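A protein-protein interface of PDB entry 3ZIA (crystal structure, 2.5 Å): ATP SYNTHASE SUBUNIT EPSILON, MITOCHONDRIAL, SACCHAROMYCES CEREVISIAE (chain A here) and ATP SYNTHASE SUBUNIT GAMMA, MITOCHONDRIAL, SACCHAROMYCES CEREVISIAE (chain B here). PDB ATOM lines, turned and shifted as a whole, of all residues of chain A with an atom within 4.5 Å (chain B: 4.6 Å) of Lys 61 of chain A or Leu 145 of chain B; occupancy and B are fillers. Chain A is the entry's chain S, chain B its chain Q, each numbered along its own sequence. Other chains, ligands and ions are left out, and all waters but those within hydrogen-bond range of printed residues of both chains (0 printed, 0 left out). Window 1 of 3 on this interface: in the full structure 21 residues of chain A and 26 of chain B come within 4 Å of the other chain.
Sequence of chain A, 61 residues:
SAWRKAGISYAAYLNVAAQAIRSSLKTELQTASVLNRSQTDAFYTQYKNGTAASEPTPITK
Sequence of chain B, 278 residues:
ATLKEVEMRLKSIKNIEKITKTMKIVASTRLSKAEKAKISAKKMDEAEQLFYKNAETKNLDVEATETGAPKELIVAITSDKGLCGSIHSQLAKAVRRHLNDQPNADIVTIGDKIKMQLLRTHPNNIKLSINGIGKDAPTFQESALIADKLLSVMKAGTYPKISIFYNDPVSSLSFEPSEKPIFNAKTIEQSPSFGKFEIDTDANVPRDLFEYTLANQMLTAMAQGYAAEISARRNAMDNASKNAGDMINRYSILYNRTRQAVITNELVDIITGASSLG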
ATOM      1  N   ASN A  15      -2.266   1.347 -18.715  1.00  0.00           N
ATOM      2  CA  ASN A  15      -2.336   2.796 -18.666  1.00  0.00           C
ATOM      3  C   ASN A  15      -0.951   3.429 -18.759  1.00  0.00           C
ATOM      4  O   ASN A  15      -0.733   4.324 -19.583  1.00  0.00           O
ATOM      5  CB  ASN A  15      -3.049   3.249 -17.395  1.00  0.00           C
ATOM      6  CG  ASN A  15      -2.964   4.741 -17.188  1.00  0.00           C
ATOM      7  OD1 ASN A  15      -2.401   5.202 -16.196  1.00  0.00           O
ATOM      8  ND2 ASN A  15      -3.504   5.507 -18.134  1.00  0.00           N
ATOM      9  N   ALA A  42      -7.986  13.526  -9.488  1.00  0.00           N
ATOM     10  CA  ALA A  42      -8.701  12.621  -8.595  1.00  0.00           C
ATOM     11  C   ALA A  42      -7.903  12.259  -7.351  1.00  0.00           C
ATOM     12  O   ALA A  42      -6.691  12.062  -7.411  1.00  0.00           O
ATOM     13  CB  ALA A  42      -9.123  11.371  -9.338  1.00  0.00           C
ATOM     14  N   TYR A  44      -8.108   9.854  -3.477  1.00  0.00           N
ATOM     15  CA  TYR A  44      -8.766   8.739  -2.799  1.00  0.00           C
ATOM     16  C   TYR A  44      -8.554   8.795  -1.293  1.00  0.00           C
ATOM     17  O   TYR A  44      -7.451   9.081  -0.819  1.00  0.00           O
ATOM     18  CB  TYR A  44      -8.341   7.384  -3.381  1.00  0.00           C
ATOM     19  CG  TYR A  44      -6.918   6.962  -3.095  1.00  0.00           C
ATOM     20  CD1 TYR A  44      -6.600   6.242  -1.935  1.00  0.00           C
ATOM     21  CD2 TYR A  44      -5.891   7.252  -3.995  1.00  0.00           C
ATOM     22  CE1 TYR A  44      -5.292   5.841  -1.669  1.00  0.00           C
ATOM     23  CE2 TYR A  44      -4.580   6.854  -3.742  1.00  0.00           C
ATOM     24  CZ  TYR A  44      -4.284   6.151  -2.578  1.00  0.00           C
ATOM     25  OH  TYR A  44      -2.983   5.764  -2.329  1.00  0.00           O
ATOM     26  N   THR A  60      -3.581  10.668  -3.650  1.00  0.00           N
ATOM     27  CA  THR A  60      -3.788  11.087  -5.028  1.00  0.00           C
ATOM     28  C   THR A  60      -3.751   9.875  -5.948  1.00  0.00           C
ATOM     29  O   THR A  60      -3.189   8.842  -5.584  1.00  0.00           O
ATOM     30  CB  THR A  60      -2.669  12.075  -5.444  1.00  0.00           C
ATOM     31  OG1 THR A  60      -2.642  13.172  -4.526  1.00  0.00           O
ATOM     32  CG2 THR A  60      -2.872  12.616  -6.857  1.00  0.00           C
ATOM     33  N   LYS A  61      -4.369   9.994  -7.124  1.00  0.00           N
ATOM     34  CA  LYS A  61      -4.046   9.118  -8.251  1.00  0.00           C
ATOM     35  C   LYS A  61      -4.668   7.737  -8.117  1.00  0.00           C
ATOM     36  O   LYS A  61      -5.604   7.412  -8.842  1.00  0.00           O
ATOM     37  CB  LYS A  61      -2.512   9.071  -8.422  1.00  0.00           C
ATOM     38  CG  LYS A  61      -1.890   7.811  -8.997  1.00  0.00           C
ATOM     39  CD  LYS A  61      -0.490   7.599  -8.408  1.00  0.00           C
ATOM     40  CE  LYS A  61      -0.435   8.039  -6.940  1.00  0.00           C
ATOM     41  NZ  LYS A  61       0.244   7.092  -6.029  1.00  0.00           N
ATOM     42  N   GLN B 141      -7.498   6.125 -17.748  1.00  0.00           N
ATOM     43  CA  GLN B 141      -6.524   6.304 -16.673  1.00  0.00           C
ATOM     44  C   GLN B 141      -7.212   6.365 -15.313  1.00  0.00           C
ATOM     45  O   GLN B 141      -6.773   5.713 -14.359  1.00  0.00           O
ATOM     46  CB  GLN B 141      -5.669   7.554 -16.885  1.00  0.00           C
ATOM     47  CG  GLN B 141      -4.583   7.723 -15.825  1.00  0.00           C
ATOM     48  CD  GLN B 141      -3.819   9.027 -15.945  1.00  0.00           C
ATOM     49  OE1 GLN B 141      -4.407  10.092 -16.121  1.00  0.00           O
ATOM     50  NE2 GLN B 141      -2.497   8.950 -15.837  1.00  0.00           N
ATOM     51  N   GLU B 142      -8.289   7.147 -15.242  1.00  0.00           N
ATOM     52  CA  GLU B 142      -9.044   7.320 -14.008  1.00  0.00           C
ATOM     53  C   GLU B 142      -9.662   6.012 -13.555  1.00  0.00           C
ATOM     54  O   GLU B 142      -9.560   5.645 -12.387  1.00  0.00           O
ATOM     55  CB  GLU B 142     -10.123   8.381 -14.189  1.00  0.00           C
ATOM     56  CG  GLU B 142      -9.630   9.792 -13.928  1.00  0.00           C
ATOM     57  CD  GLU B 142     -10.503  10.871 -14.554  1.00  0.00           C
ATOM     58  OE1 GLU B 142     -11.601  10.555 -15.067  1.00  0.00           O
ATOM     59  OE2 GLU B 142     -10.080  12.048 -14.533  1.00  0.00           O
ATOM     60  N   SER B 143     -10.277   5.305 -14.497  1.00  0.00           N
ATOM     61  CA  SER B 143     -10.913   4.026 -14.216  1.00  0.00           C
ATOM     62  C   SER B 143      -9.907   2.992 -13.711  1.00  0.00           C
ATOM     63  O   SER B 143     -10.106   2.385 -12.651  1.00  0.00           O
ATOM     64  CB  SER B 143     -11.617   3.516 -15.468  1.00  0.00           C
ATOM     65  OG  SER B 143     -12.602   2.568 -15.112  1.00  0.00           O
ATOM     66  N   ALA B 144      -8.823   2.829 -14.471  1.00  0.00           N
ATOM     67  CA  ALA B 144      -7.746   1.887 -14.165  1.00  0.00           C
ATOM     68  C   ALA B 144      -7.128   2.127 -12.798  1.00  0.00           C
ATOM     69  O   ALA B 144      -6.930   1.189 -12.034  1.00  0.00           O
ATOM     70  CB  ALA B 144      -6.676   1.936 -15.242  1.00  0.00           C
ATOM     71  N   LEU B 145      -6.830   3.385 -12.495  1.00  0.00           N
ATOM     72  CA  LEU B 145      -6.206   3.755 -11.222  1.00  0.00           C
ATOM     73  C   LEU B 145      -7.140   3.544 -10.027  1.00  0.00           C
ATOM     74  O   LEU B 145      -6.690   3.191  -8.933  1.00  0.00           O
ATOM     75  CB  LEU B 145      -5.708   5.205 -11.268  1.00  0.00           C
ATOM     76  CG  LEU B 145      -4.263   5.539 -11.676  1.00  0.00           C
ATOM     77  CD1 LEU B 145      -3.788   4.799 -12.925  1.00  0.00           C
ATOM     78  CD2 LEU B 145      -4.136   7.036 -11.880  1.00  0.00           C
ATOM     79  N   ILE B 146      -8.436   3.774 -10.250  1.00  0.00           N
ATOM     80  CA  ILE B 146      -9.472   3.487  -9.253  1.00  0.00           C
ATOM     81  C   ILE B 146      -9.583   1.973  -9.057  1.00  0.00           C
ATOM     82  O   ILE B 146      -9.535   1.490  -7.922  1.00  0.00           O
ATOM     83  CB  ILE B 146     -10.848   4.100  -9.646  1.00  0.00           C
ATOM     84  CG1 ILE B 146     -10.832   5.618  -9.448  1.00  0.00           C
ATOM     85  CG2 ILE B 146     -11.985   3.481  -8.826  1.00  0.00           C
ATOM     86  CD1 ILE B 146     -11.912   6.358 -10.224  1.00  0.00           C
ATOM     87  N   ALA B 147      -9.718   1.245 -10.169  1.00  0.00           N
ATOM     88  CA  ALA B 147      -9.696  -0.219 -10.167  1.00  0.00           C
ATOM     89  C   ALA B 147      -8.467  -0.740  -9.426  1.00  0.00           C
ATOM     90  O   ALA B 147      -8.580  -1.610  -8.557  1.00  0.00           O
ATOM     91  CB  ALA B 147      -9.736  -0.760 -11.599  1.00  0.00           C
ATOM     92  N   ASP B 148      -7.305  -0.180  -9.760  1.00  0.00           N
ATOM     93  CA  ASP B 148      -6.053  -0.527  -9.101  1.00  0.00           C
ATOM     94  C   ASP B 148      -6.177  -0.445  -7.581  1.00  0.00           C
ATOM     95  O   ASP B 148      -5.908  -1.427  -6.884  1.00  0.00           O
ATOM     96  CB  ASP B 148      -4.910   0.371  -9.581  1.00  0.00           C
ATOM     97  CG  ASP B 148      -3.547  -0.161  -9.175  1.00  0.00           C
ATOM     98  OD1 ASP B 148      -3.095  -1.151  -9.785  1.00  0.00           O
ATOM     99  OD2 ASP B 148      -2.932   0.397  -8.242  1.00  0.00           O
ATOM    100  N   LYS B 149      -6.595   0.713  -7.077  1.00  0.00           N
ATOM    101  CA  LYS B 149      -6.736   0.916  -5.637  1.00  0.00           C
ATOM    102  C   LYS B 149      -7.864   0.075  -5.032  1.00  0.00           C
ATOM    103  O   LYS B 149      -7.809  -0.290  -3.853  1.00  0.00           O
ATOM    104  CB  LYS B 149      -6.897   2.406  -5.300  1.00  0.00           C
ATOM    105  CG  LYS B 149      -5.613   3.242  -5.450  1.00  0.00           C
ATOM    106  CD  LYS B 149      -4.396   2.575  -4.772  1.00  0.00           C
ATOM    107  CE  LYS B 149      -3.185   3.503  -4.641  1.00  0.00           C
ATOM    108  NZ  LYS B 149      -2.669   4.046  -5.933  1.00  0.00           N
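Of the printed residues of chain B, Asn 15 of chain A touches Gln 141 (3.2 Å) and Leu 145 (3.6 Å). Of the printed residues of chain B, Tyr 44 of chain A touches Lys 149. Thr 60 of chain A touches none of the printed residues of chain B. Of chain A, only Asn 15 (3.6 Å) and Lys 61 (3.3 Å) come within 4 Å of Leu 145 of chain B. Ala 147 of chain B touches none of the printed residues of chain A. Printed residues of chain A within 4 Å of Lys 149 of chain B: Tyr 44. The nearest printed residue of chain B that does not touch Asn 15 of chain A is Ala 144 of chain B (4.4 Å).
Among the printed residues, merely in contact across the chains: Asn 15 of chain A with Gln 141 of chain B, Tyr 44 of chain A with Lys 149 of chain B, Lys 61 of chain A with Leu 145 of chain B and Asn 15 of chain A with Leu 145 of chain B.
The backbone carbonyl oxygen (O) of Ala 42 of chain A sits at hydrogen-bond distance from the backbone NH (N) of Lys 61 of chain A, 3.1 Å away.
Of the 5 printed residues of chain A, 3 touch a printed residue of chain B.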
